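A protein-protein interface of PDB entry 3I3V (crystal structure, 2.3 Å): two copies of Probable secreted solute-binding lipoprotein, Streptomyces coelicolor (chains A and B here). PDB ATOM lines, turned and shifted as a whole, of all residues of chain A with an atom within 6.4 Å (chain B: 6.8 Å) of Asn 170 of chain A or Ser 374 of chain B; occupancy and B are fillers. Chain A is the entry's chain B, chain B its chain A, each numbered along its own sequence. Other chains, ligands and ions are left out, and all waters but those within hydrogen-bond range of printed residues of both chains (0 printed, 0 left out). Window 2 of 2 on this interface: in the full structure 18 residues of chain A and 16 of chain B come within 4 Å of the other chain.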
ATOM      1  N   VAL A 167     -23.175 -28.339 -12.530  1.00  0.00           N
ATOM      2  CA  VAL A 167     -24.417 -28.282 -13.282  1.00  0.00           C
ATOM      3  C   VAL A 167     -24.783 -26.831 -13.553  1.00  0.00           C
ATOM      4  O   VAL A 167     -24.476 -25.950 -12.748  1.00  0.00           O
ATOM      5  CB  VAL A 167     -25.574 -28.942 -12.490  1.00  0.00           C
ATOM      6  CG1 VAL A 167     -25.755 -28.243 -11.162  1.00  0.00           C
ATOM      7  CG2 VAL A 167     -26.870 -28.870 -13.285  1.00  0.00           C
ATOM      8  N   GLY A 168     -25.437 -26.588 -14.686  1.00  0.00           N
ATOM      9  CA  GLY A 168     -25.846 -25.240 -15.028  1.00  0.00           C
ATOM     10  C   GLY A 168     -27.079 -24.854 -14.236  1.00  0.00           C
ATOM     11  O   GLY A 168     -28.204 -25.006 -14.702  1.00  0.00           O
ATOM     12  N   GLY A 169     -26.870 -24.359 -13.025  1.00  0.00           N
ATOM     13  CA  GLY A 169     -27.987 -23.980 -12.192  1.00  0.00           C
ATOM     14  C   GLY A 169     -28.912 -22.943 -12.804  1.00  0.00           C
ATOM     15  O   GLY A 169     -30.109 -22.935 -12.500  1.00  0.00           O
ATOM     16  N   ASN A 170     -28.384 -22.079 -13.671  1.00  0.00           N
ATOM     17  CA  ASN A 170     -29.218 -21.040 -14.262  1.00  0.00           C
ATOM     18  C   ASN A 170     -29.741 -21.300 -15.663  1.00  0.00           C
ATOM     19  O   ASN A 170     -30.102 -20.364 -16.366  1.00  0.00           O
ATOM     20  CB  ASN A 170     -28.490 -19.690 -14.235  1.00  0.00           C
ATOM     21  CG  ASN A 170     -29.439 -18.515 -14.420  1.00  0.00           C
ATOM     22  OD1 ASN A 170     -30.630 -18.640 -14.173  1.00  0.00           O
ATOM     23  ND2 ASN A 170     -28.912 -17.375 -14.836  1.00  0.00           N
ATOM     24  N   ASP A 171     -29.787 -22.558 -16.081  1.00  0.00           N
ATOM     25  CA  ASP A 171     -30.310 -22.867 -17.403  1.00  0.00           C
ATOM     26  C   ASP A 171     -30.917 -24.264 -17.490  1.00  0.00           C
ATOM     27  O   ASP A 171     -31.061 -24.958 -16.482  1.00  0.00           O
ATOM     28  CB  ASP A 171     -29.229 -22.678 -18.472  1.00  0.00           C
ATOM     29  CG  ASP A 171     -28.250 -23.837 -18.544  1.00  0.00           C
ATOM     30  OD1 ASP A 171     -28.419 -24.845 -17.823  1.00  0.00           O
ATOM     31  OD2 ASP A 171     -27.296 -23.736 -19.350  1.00  0.00           O
ATOM     32  N   TRP A 172     -31.268 -24.676 -18.702  1.00  0.00           N
ATOM     33  CA  TRP A 172     -31.888 -25.973 -18.918  1.00  0.00           C
ATOM     34  C   TRP A 172     -31.220 -27.189 -18.249  1.00  0.00           C
ATOM     35  O   TRP A 172     -31.917 -28.112 -17.819  1.00  0.00           O
ATOM     36  CB  TRP A 172     -32.034 -26.239 -20.421  1.00  0.00           C
ATOM     37  CG  TRP A 172     -30.730 -26.361 -21.167  1.00  0.00           C
ATOM     38  CD1 TRP A 172     -29.963 -25.343 -21.661  1.00  0.00           C
ATOM     39  CD2 TRP A 172     -30.047 -27.576 -21.509  1.00  0.00           C
ATOM     40  NE1 TRP A 172     -28.849 -25.848 -22.294  1.00  0.00           N
ATOM     41  CE2 TRP A 172     -28.877 -27.216 -22.214  1.00  0.00           C
ATOM     42  CE3 TRP A 172     -30.315 -28.935 -21.291  1.00  0.00           C
ATOM     43  CZ2 TRP A 172     -27.973 -28.165 -22.703  1.00  0.00           C
ATOM     44  CZ3 TRP A 172     -29.419 -29.880 -21.779  1.00  0.00           C
ATOM     45  CH2 TRP A 172     -28.261 -29.489 -22.478  1.00  0.00           C
ATOM     46  N   THR A 173     -29.893 -27.221 -18.169  1.00  0.00           N
ATOM     47  CA  THR A 173     -29.248 -28.375 -17.550  1.00  0.00           C
ATOM     48  C   THR A 173     -29.641 -28.462 -16.080  1.00  0.00           C
ATOM     49  O   THR A 173     -29.931 -29.538 -15.567  1.00  0.00           O
ATOM     50  CB  THR A 173     -27.706 -28.325 -17.695  1.00  0.00           C
ATOM     51  OG1 THR A 173     -27.193 -27.121 -17.115  1.00  0.00           O
ATOM     52  CG2 THR A 173     -27.322 -28.387 -19.171  1.00  0.00           C
ATOM     53  N   GLY A 174     -29.677 -27.321 -15.411  1.00  0.00           N
ATOM     54  CA  GLY A 174     -30.072 -27.316 -14.016  1.00  0.00           C
ATOM     55  C   GLY A 174     -31.542 -27.686 -13.870  1.00  0.00           C
ATOM     56  O   GLY A 174     -31.887 -28.524 -13.036  1.00  0.00           O
ATOM     57  N   ALA A 225     -23.547 -22.736  -7.967  1.00  0.00           N
ATOM     58  CA  ALA A 225     -24.183 -23.469  -9.056  1.00  0.00           C
ATOM     59  C   ALA A 225     -25.384 -22.718  -9.645  1.00  0.00           C
ATOM     60  O   ALA A 225     -25.640 -22.806 -10.845  1.00  0.00           O
ATOM     61  CB  ALA A 225     -24.615 -24.849  -8.576  1.00  0.00           C
ATOM     62  N   GLN A 226     -26.109 -21.981  -8.802  1.00  0.00           N
ATOM     63  CA  GLN A 226     -27.287 -21.231  -9.245  1.00  0.00           C
ATOM     64  C   GLN A 226     -27.009 -20.282 -10.411  1.00  0.00           C
ATOM     65  O   GLN A 226     -27.912 -19.959 -11.184  1.00  0.00           O
ATOM     66  CB  GLN A 226     -27.890 -20.433  -8.082  1.00  0.00           C
ATOM     67  CG  GLN A 226     -27.006 -19.309  -7.561  1.00  0.00           C
ATOM     68  CD  GLN A 226     -26.070 -19.757  -6.456  1.00  0.00           C
ATOM     69  OE1 GLN A 226     -25.593 -20.893  -6.447  1.00  0.00           O
ATOM     70  NE2 GLN A 226     -25.787 -18.853  -5.523  1.00  0.00           N
ATOM     71  N   GLY A 227     -25.762 -19.839 -10.543  1.00  0.00           N
ATOM     72  CA  GLY A 227     -25.422 -18.936 -11.629  1.00  0.00           C
ATOM     73  C   GLY A 227     -24.697 -19.580 -12.804  1.00  0.00           C
ATOM     74  O   GLY A 227     -24.327 -18.890 -13.746  1.00  0.00           O
ATOM     75  N   LEU A 228     -24.505 -20.896 -12.767  1.00  0.00           N
ATOM     76  CA  LEU A 228     -23.797 -21.591 -13.844  1.00  0.00           C
ATOM     77  C   LEU A 228     -24.683 -21.983 -15.031  1.00  0.00           C
ATOM     78  O   LEU A 228     -25.911 -21.998 -14.931  1.00  0.00           O
ATOM     79  CB  LEU A 228     -23.117 -22.844 -13.292  1.00  0.00           C
ATOM     80  CG  LEU A 228     -22.065 -22.628 -12.207  1.00  0.00           C
ATOM     81  CD1 LEU A 228     -21.619 -23.979 -11.666  1.00  0.00           C
ATOM     82  CD2 LEU A 228     -20.886 -21.851 -12.784  1.00  0.00           C
ATOM     83  N   THR A 229     -24.039 -22.311 -16.150  1.00  0.00           N
ATOM     84  CA  THR A 229     -24.737 -22.714 -17.362  1.00  0.00           C
ATOM     85  C   THR A 229     -24.111 -23.981 -17.907  1.00  0.00           C
ATOM     86  O   THR A 229     -23.175 -24.521 -17.321  1.00  0.00           O
ATOM     87  CB  THR A 229     -24.620 -21.652 -18.469  1.00  0.00           C
ATOM     88  OG1 THR A 229     -23.292 -21.677 -18.999  1.00  0.00           O
ATOM     89  CG2 THR A 229     -24.900 -20.259 -17.915  1.00  0.00           C
ATOM     90  N   GLN A 367     -39.489 -20.928 -19.222  1.00  0.00           N
ATOM     91  CA  GLN A 367     -38.477 -19.975 -18.768  1.00  0.00           C
ATOM     92  C   GLN A 367     -38.600 -19.714 -17.269  1.00  0.00           C
ATOM     93  O   GLN A 367     -37.596 -19.672 -16.563  1.00  0.00           O
ATOM     94  CB  GLN A 367     -38.583 -18.658 -19.552  1.00  0.00           C
ATOM     95  CG  GLN A 367     -37.560 -17.595 -19.155  1.00  0.00           C
ATOM     96  CD  GLN A 367     -36.126 -18.112 -19.167  1.00  0.00           C
ATOM     97  OE1 GLN A 367     -35.676 -18.714 -20.145  1.00  0.00           O
ATOM     98  NE2 GLN A 367     -35.398 -17.869 -18.076  1.00  0.00           N
ATOM     99  N   ILE A 370     -36.953 -22.285 -15.101  1.00  0.00           N
ATOM    100  CA  ILE A 370     -35.497 -22.226 -15.048  1.00  0.00           C
ATOM    101  C   ILE A 370     -35.052 -21.185 -14.025  1.00  0.00           C
ATOM    102  O   ILE A 370     -34.070 -21.366 -13.309  1.00  0.00           O
ATOM    103  CB  ILE A 370     -34.938 -21.876 -16.446  1.00  0.00           C
ATOM    104  CG1 ILE A 370     -35.204 -23.050 -17.393  1.00  0.00           C
ATOM    105  CG2 ILE A 370     -33.452 -21.523 -16.367  1.00  0.00           C
ATOM    106  CD1 ILE A 370     -34.801 -22.807 -18.832  1.00  0.00           C
ATOM    107  N   THR A 371     -35.792 -20.089 -13.963  1.00  0.00           N
ATOM    108  CA  THR A 371     -35.505 -19.013 -13.025  1.00  0.00           C
ATOM    109  C   THR A 371     -35.758 -19.507 -11.595  1.00  0.00           C
ATOM    110  O   THR A 371     -35.027 -19.153 -10.668  1.00  0.00           O
ATOM    111  CB  THR A 371     -36.395 -17.798 -13.334  1.00  0.00           C
ATOM    112  OG1 THR A 371     -36.138 -17.356 -14.674  1.00  0.00           O
ATOM    113  CG2 THR A 371     -36.113 -16.665 -12.371  1.00  0.00           C
ATOM    114  N   THR A 373     -35.563 -22.667 -10.778  1.00  0.00           N
ATOM    115  CA  THR A 373     -34.574 -23.709 -10.535  1.00  0.00           C
ATOM    116  C   THR A 373     -33.321 -23.032  -9.992  1.00  0.00           C
ATOM    117  O   THR A 373     -32.741 -23.470  -9.004  1.00  0.00           O
ATOM    118  CB  THR A 373     -34.223 -24.465 -11.830  1.00  0.00           C
ATOM    119  OG1 THR A 373     -35.382 -25.159 -12.315  1.00  0.00           O
ATOM    120  CG2 THR A 373     -33.112 -25.467 -11.568  1.00  0.00           C
ATOM    121  N   SER A 374     -32.921 -21.947 -10.644  1.00  0.00           N
ATOM    122  CA  SER A 374     -31.753 -21.178 -10.237  1.00  0.00           C
ATOM    123  C   SER A 374     -31.910 -20.670  -8.814  1.00  0.00           C
ATOM    124  O   SER A 374     -30.938 -20.587  -8.073  1.00  0.00           O
ATOM    125  CB  SER A 374     -31.547 -19.987 -11.171  1.00  0.00           C
ATOM    126  OG  SER A 374     -30.481 -19.177 -10.721  1.00  0.00           O
ATOM    127  N   PHE A 377     -31.338 -23.780  -6.481  1.00  0.00           N
ATOM    128  CA  PHE A 377     -29.966 -24.269  -6.297  1.00  0.00           C
ATOM    129  C   PHE A 377     -29.182 -23.397  -5.333  1.00  0.00           C
ATOM    130  O   PHE A 377     -28.024 -23.675  -5.027  1.00  0.00           O
ATOM    131  CB  PHE A 377     -29.214 -24.314  -7.629  1.00  0.00           C
ATOM    132  CG  PHE A 377     -29.317 -25.626  -8.337  1.00  0.00           C
ATOM    133  CD1 PHE A 377     -30.379 -25.893  -9.198  1.00  0.00           C
ATOM    134  CD2 PHE A 377     -28.334 -26.599  -8.161  1.00  0.00           C
ATOM    135  CE1 PHE A 377     -30.456 -27.114  -9.874  1.00  0.00           C
ATOM    136  CE2 PHE A 377     -28.405 -27.819  -8.829  1.00  0.00           C
ATOM    137  CZ  PHE A 377     -29.462 -28.075  -9.688  1.00  0.00           C
ATOM    138  N   GLY B 169     -32.534  -9.208 -11.749  1.00  0.00           N
ATOM    139  CA  GLY B 169     -31.375  -9.488 -12.562  1.00  0.00           C
ATOM    140  C   GLY B 169     -31.431 -10.851 -13.229  1.00  0.00           C
ATOM    141  O   GLY B 169     -30.692 -11.096 -14.176  1.00  0.00           O
ATOM    142  N   ASN B 170     -32.299 -11.742 -12.759  1.00  0.00           N
ATOM    143  CA  ASN B 170     -32.376 -13.060 -13.376  1.00  0.00           C
ATOM    144  C   ASN B 170     -33.643 -13.359 -14.167  1.00  0.00           C
ATOM    145  O   ASN B 170     -34.012 -14.521 -14.318  1.00  0.00           O
ATOM    146  CB  ASN B 170     -32.155 -14.166 -12.336  1.00  0.00           C
ATOM    147  CG  ASN B 170     -31.790 -15.495 -12.981  1.00  0.00           C
ATOM    148  OD1 ASN B 170     -31.129 -15.524 -14.021  1.00  0.00           O
ATOM    149  ND2 ASN B 170     -32.200 -16.592 -12.369  1.00  0.00           N
ATOM    150  N   ASP B 171     -34.324 -12.324 -14.648  1.00  0.00           N
ATOM    151  CA  ASP B 171     -35.506 -12.536 -15.483  1.00  0.00           C
ATOM    152  C   ASP B 171     -35.743 -11.379 -16.463  1.00  0.00           C
ATOM    153  O   ASP B 171     -34.863 -10.530 -16.650  1.00  0.00           O
ATOM    154  CB  ASP B 171     -36.758 -12.846 -14.635  1.00  0.00           C
ATOM    155  CG  ASP B 171     -37.343 -11.631 -13.932  1.00  0.00           C
ATOM    156  OD1 ASP B 171     -36.887 -10.489 -14.163  1.00  0.00           O
ATOM    157  OD2 ASP B 171     -38.289 -11.831 -13.134  1.00  0.00           O
ATOM    158  N   LEU B 178     -31.155  -3.835 -18.789  1.00  0.00           N
ATOM    159  CA  LEU B 178     -29.797  -3.927 -19.320  1.00  0.00           C
ATOM    160  C   LEU B 178     -29.823  -3.352 -20.733  1.00  0.00           C
ATOM    161  O   LEU B 178     -29.001  -2.508 -21.095  1.00  0.00           O
ATOM    162  CB  LEU B 178     -29.347  -5.393 -19.389  1.00  0.00           C
ATOM    163  CG  LEU B 178     -27.866  -5.756 -19.224  1.00  0.00           C
ATOM    164  CD1 LEU B 178     -27.571  -7.021 -20.008  1.00  0.00           C
ATOM    165  CD2 LEU B 178     -26.976  -4.612 -19.698  1.00  0.00           C
ATOM    166  N   ALA B 225     -28.375  -8.565  -6.995  1.00  0.00           N
ATOM    167  CA  ALA B 225     -29.380  -8.331  -8.026  1.00  0.00           C
ATOM    168  C   ALA B 225     -29.422  -9.394  -9.134  1.00  0.00           C
ATOM    169  O   ALA B 225     -30.468  -9.596  -9.747  1.00  0.00           O
ATOM    170  CB  ALA B 225     -29.174  -6.957  -8.645  1.00  0.00           C
ATOM    171  N   GLN B 226     -28.305 -10.071  -9.394  1.00  0.00           N
ATOM    172  CA  GLN B 226     -28.279 -11.080 -10.453  1.00  0.00           C
ATOM    173  C   GLN B 226     -29.192 -12.261 -10.170  1.00  0.00           C
ATOM    174  O   GLN B 226     -29.445 -13.075 -11.049  1.00  0.00           O
ATOM    175  CB  GLN B 226     -26.857 -11.600 -10.694  1.00  0.00           C
ATOM    176  CG  GLN B 226     -26.247 -12.370  -9.532  1.00  0.00           C
ATOM    177  CD  GLN B 226     -25.494 -11.477  -8.576  1.00  0.00           C
ATOM    178  OE1 GLN B 226     -25.885 -10.334  -8.327  1.00  0.00           O
ATOM    179  NE2 GLN B 226     -24.409 -11.997  -8.020  1.00  0.00           N
ATOM    180  N   GLY B 227     -29.697 -12.345  -8.946  1.00  0.00           N
ATOM    181  CA  GLY B 227     -30.566 -13.453  -8.589  1.00  0.00           C
ATOM    182  C   GLY B 227     -32.012 -13.063  -8.335  1.00  0.00           C
ATOM    183  O   GLY B 227     -32.851 -13.938  -8.124  1.00  0.00           O
ATOM    184  N   GLN B 367     -34.333 -16.834 -24.357  1.00  0.00           N
ATOM    185  CA  GLN B 367     -33.971 -17.425 -23.072  1.00  0.00           C
ATOM    186  C   GLN B 367     -32.494 -17.238 -22.731  1.00  0.00           C
ATOM    187  O   GLN B 367     -32.159 -16.861 -21.609  1.00  0.00           O
ATOM    188  CB  GLN B 367     -34.324 -18.911 -23.027  1.00  0.00           C
ATOM    189  CG  GLN B 367     -35.813 -19.181 -23.078  1.00  0.00           C
ATOM    190  CD  GLN B 367     -36.212 -20.441 -22.318  1.00  0.00           C
ATOM    191  OE1 GLN B 367     -37.340 -20.923 -22.445  1.00  0.00           O
ATOM    192  NE2 GLN B 367     -35.289 -20.973 -21.514  1.00  0.00           N
ATOM    193  N   LEU B 369     -30.549 -14.969 -23.628  1.00  0.00           N
ATOM    194  CA  LEU B 369     -30.347 -13.560 -23.331  1.00  0.00           C
ATOM    195  C   LEU B 369     -30.697 -13.262 -21.870  1.00  0.00           C
ATOM    196  O   LEU B 369     -30.094 -12.386 -21.253  1.00  0.00           O
ATOM    197  CB  LEU B 369     -31.185 -12.719 -24.291  1.00  0.00           C
ATOM    198  CG  LEU B 369     -30.642 -11.373 -24.766  1.00  0.00           C
ATOM    199  CD1 LEU B 369     -29.173 -11.477 -25.154  1.00  0.00           C
ATOM    200  CD2 LEU B 369     -31.482 -10.922 -25.954  1.00  0.00           C
ATOM    201  N   ILE B 370     -31.661 -13.990 -21.310  1.00  0.00           N
ATOM    202  CA  ILE B 370     -32.034 -13.802 -19.907  1.00  0.00           C
ATOM    203  C   ILE B 370     -30.854 -14.300 -19.065  1.00  0.00           C
ATOM    204  O   ILE B 370     -30.424 -13.650 -18.109  1.00  0.00           O
ATOM    205  CB  ILE B 370     -33.286 -14.646 -19.515  1.00  0.00           C
ATOM    206  CG1 ILE B 370     -34.511 -14.205 -20.321  1.00  0.00           C
ATOM    207  CG2 ILE B 370     -33.559 -14.509 -18.022  1.00  0.00           C
ATOM    208  CD1 ILE B 370     -35.045 -12.855 -19.951  1.00  0.00           C
ATOM    209  N   THR B 371     -30.343 -15.469 -19.435  1.00  0.00           N
ATOM    210  CA  THR B 371     -29.223 -16.075 -18.730  1.00  0.00           C
ATOM    211  C   THR B 371     -28.000 -15.162 -18.770  1.00  0.00           C
ATOM    212  O   THR B 371     -27.364 -14.928 -17.744  1.00  0.00           O
ATOM    213  CB  THR B 371     -28.879 -17.447 -19.342  1.00  0.00           C
ATOM    214  OG1 THR B 371     -30.038 -18.292 -19.290  1.00  0.00           O
ATOM    215  CG2 THR B 371     -27.751 -18.105 -18.581  1.00  0.00           C
ATOM    216  N   ALA B 372     -27.682 -14.630 -19.949  1.00  0.00           N
ATOM    217  CA  ALA B 372     -26.538 -13.733 -20.105  1.00  0.00           C
ATOM    218  C   ALA B 372     -26.716 -12.457 -19.278  1.00  0.00           C
ATOM    219  O   ALA B 372     -25.742 -11.803 -18.915  1.00  0.00           O
ATOM    220  CB  ALA B 372     -26.352 -13.375 -21.571  1.00  0.00           C
ATOM    221  N   THR B 373     -27.964 -12.106 -18.988  1.00  0.00           N
ATOM    222  CA  THR B 373     -28.257 -10.909 -18.208  1.00  0.00           C
ATOM    223  C   THR B 373     -27.859 -11.102 -16.746  1.00  0.00           C
ATOM    224  O   THR B 373     -27.233 -10.236 -16.141  1.00  0.00           O
ATOM    225  CB  THR B 373     -29.763 -10.532 -18.290  1.00  0.00           C
ATOM    226  OG1 THR B 373     -30.073 -10.079 -19.619  1.00  0.00           O
ATOM    227  CG2 THR B 373     -30.097  -9.432 -17.289  1.00  0.00           C
ATOM    228  N   SER B 374     -28.215 -12.249 -16.185  1.00  0.00           N
ATOM    229  CA  SER B 374     -27.883 -12.557 -14.802  1.00  0.00           C
ATOM    230  C   SER B 374     -26.365 -12.488 -14.617  1.00  0.00           C
ATOM    231  O   SER B 374     -25.869 -11.847 -13.688  1.00  0.00           O
ATOM    232  CB  SER B 374     -28.399 -13.953 -14.453  1.00  0.00           C
ATOM    233  OG  SER B 374     -28.018 -14.320 -13.140  1.00  0.00           O
ATOM    234  N   THR B 375     -25.639 -13.151 -15.512  1.00  0.00           N
ATOM    235  CA  THR B 375     -24.181 -13.158 -15.472  1.00  0.00           C
ATOM    236  C   THR B 375     -23.689 -11.708 -15.490  1.00  0.00           C
ATOM    237  O   THR B 375     -22.781 -11.332 -14.754  1.00  0.00           O
ATOM    238  CB  THR B 375     -23.587 -13.882 -16.704  1.00  0.00           C
ATOM    239  OG1 THR B 375     -24.033 -15.249 -16.734  1.00  0.00           O
ATOM    240  CG2 THR B 375     -22.065 -13.844 -16.659  1.00  0.00           C
ATOM    241  N   SER B 376     -24.312 -10.893 -16.334  1.00  0.00           N
ATOM    242  CA  SER B 376     -23.941  -9.497 -16.464  1.00  0.00           C
ATOM    243  C   SER B 376     -24.212  -8.601 -15.257  1.00  0.00           C
ATOM    244  O   SER B 376     -23.505  -7.615 -15.074  1.00  0.00           O
ATOM    245  CB  SER B 376     -24.615  -8.904 -17.691  1.00  0.00           C
ATOM    246  OG  SER B 376     -24.114  -9.515 -18.862  1.00  0.00           O
ATOM    247  N   PHE B 377     -25.223  -8.915 -14.445  1.00  0.00           N
ATOM    248  CA  PHE B 377     -25.521  -8.081 -13.275  1.00  0.00           C
ATOM    249  C   PHE B 377     -24.583  -8.396 -12.118  1.00  0.00           C
ATOM    250  O   PHE B 377     -24.579  -7.706 -11.098  1.00  0.00           O
ATOM    251  CB  PHE B 377     -26.975  -8.260 -12.802  1.00  0.00           C
ATOM    252  CG  PHE B 377     -27.915  -7.211 -13.329  1.00  0.00           C
ATOM    253  CD1 PHE B 377     -28.582  -7.395 -14.537  1.00  0.00           C
ATOM    254  CD2 PHE B 377     -28.099  -6.013 -12.637  1.00  0.00           C
ATOM    255  CE1 PHE B 377     -29.409  -6.380 -15.067  1.00  0.00           C
ATOM    256  CE2 PHE B 377     -28.916  -4.998 -13.150  1.00  0.00           C
ATOM    257  CZ  PHE B 377     -29.581  -5.182 -14.367  1.00  0.00           C
ATOM    258  N   THR B 378     -23.793  -9.450 -12.281  1.00  0.00           N
ATOM    259  CA  THR B 378     -22.849  -9.851 -11.257  1.00  0.00           C
ATOM    260  C   THR B 378     -21.696  -8.861 -11.227  1.00  0.00           C
ATOM    261  O   THR B 378     -21.036  -8.625 -12.240  1.00  0.00           O
ATOM    262  CB  THR B 378     -22.319 -11.255 -11.537  1.00  0.00           C
ATOM    263  OG1 THR B 378     -23.419 -12.170 -11.534  1.00  0.00           O
ATOM    264  CG2 THR B 378     -21.302 -11.668 -10.471  1.00  0.00           C
ATOM    265  N   ARG B 379     -21.470  -8.285 -10.052  1.00  0.00           N
ATOM    266  CA  ARG B 379     -20.423  -7.297  -9.857  1.00  0.00           C
ATOM    267  C   ARG B 379     -19.010  -7.753 -10.189  1.00  0.00           C
ATOM    268  O   ARG B 379     -18.532  -8.764  -9.683  1.00  0.00           O
ATOM    269  CB  ARG B 379     -20.475  -6.776  -8.423  1.00  0.00           C
ATOM    270  CG  ARG B 379     -20.959  -5.350  -8.363  1.00  0.00           C
ATOM    271  CD  ARG B 379     -21.372  -4.953  -6.985  1.00  0.00           C
ATOM    272  NE  ARG B 379     -20.695  -3.732  -6.583  1.00  0.00           N
ATOM    273  CZ  ARG B 379     -20.985  -3.048  -5.485  1.00  0.00           C
ATOM    274  NH1 ARG B 379     -21.954  -3.471  -4.679  1.00  0.00           N
ATOM    275  NH2 ARG B 379     -20.299  -1.948  -5.191  1.00  0.00           N
ATOM    276  N   THR B 381     -17.948  -8.297 -13.448  1.00  0.00           N
ATOM    277  CA  THR B 381     -17.895  -8.952 -14.761  1.00  0.00           C
ATOM    278  C   THR B 381     -17.466  -7.943 -15.817  1.00  0.00           C
ATOM    279  O   THR B 381     -18.215  -7.032 -16.158  1.00  0.00           O
ATOM    280  CB  THR B 381     -19.268  -9.531 -15.151  1.00  0.00           C
ATOM    281  OG1 THR B 381     -19.713 -10.432 -14.130  1.00  0.00           O
ATOM    282  CG2 THR B 381     -19.173 -10.288 -16.465  1.00  0.00           C
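The side-chain amide oxygen (OE1) of Gln 367 of chain A is in hydrogen-bond range of the side-chain amide nitrogen (NE2) of Gln 367 of chain B (2.7 Å). ND2 of Asn 170 of chain A is in hydrogen-bond range of OD1 of Asn 170 of chain B.
The side-chain amide oxygen (OD1) of Asn 170 of chain A lies close to the side-chain hydroxyl (OG) of Ser 374 of chain A (3.5 Å). OG1 of Thr 375 of chain B lies within hydrogen-bond range of O of Thr 371 of chain B, at 3.5 Å. O of Leu 228 of chain A sits at hydrogen-bond distance from N of Asn 170 of chain A (2.8 Å). O of Gln 367 of chain A sits at hydrogen-bond distance from OG1 of Thr 371 of chain A, at 3.3 Å. OG of Ser 374 of chain B lies within hydrogen-bond range of O of Gln 226 of chain B (2.8 Å). The backbone carbonyl oxygen (O) of Ser 374 of chain B is in hydrogen-bond range of the side-chain hydroxyl (OG1) of Thr 378 of chain B (3.3 Å).
Among the printed residues, pairs that only touch across the chains: Ile 370 of chain A with Gln 367 of chain B (3.3 Å), Asn 170 of chain A with Ser 374 of chain B (3.5 Å), Ser 374 of chain A with Asn 170 of chain B (3.5 Å), Thr 371 of chain A with Asn 170 of chain B (3.6 Å), Asn 170 of chain A with Thr 371 of chain B (3.6 Å), Thr 229 of chain A with Thr 371 of chain B (3.6 Å) and Gln 367 of chain A with Ile 370 of chain B (3.8 Å).
Asn 170 of chain A touches just these residues of chain B: Asn 170, Thr 371 and Ser 374. Of chain A, only Asn 170 comes within 4 Å of Ser 374 of chain B. Of the printed residues of chain B, Thr 229 of chain A touches Thr 371. Of the printed residues of chain A, Ile 370 of chain B touches Gln 367 (3.8 Å). Gly 227 of chain B touches none of the printed residues of chain A. The nearest residue of chain A that does not touch Ser 374 of chain B is Gly 227 of chain A (5.5 Å). The nearest printed residue of chain A that does not touch Gln 367 of chain B is Trp 172 of chain A (6.1 Å).
Of the 20 printed residues of chain B, 5 touch a printed residue of chain A. Hydrophobic or aromatic side chains of chain B within 4 Å of the printed part of chain A: Ile 370. Among the printed residues, no Asp or Glu carboxylate lies within 4 Å of a Lys or Arg side-chain nitrogen of the other chain.
Asn 170 of chain A touches Thr 371 of chain B, and with the chains exchanged Thr 371 of chain A touches Asn 170 of chain B. Asn 170 of chain A touches Ser 374 of chain B, and with the chains exchanged Ser 374 of chain A touches Asn 170 of chain B. Gln 367 of chain B touches its own counterpart, Gln 367 of chain A. Gln 367 of chain A touches Ile 370 of chain B, and with the chains exchanged Ile 370 of chain A touches Gln 367 of chain B. Of the 9 pairs that touch across the chains among the printed residues, 8 have their exchanged pair printed and touching as well.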
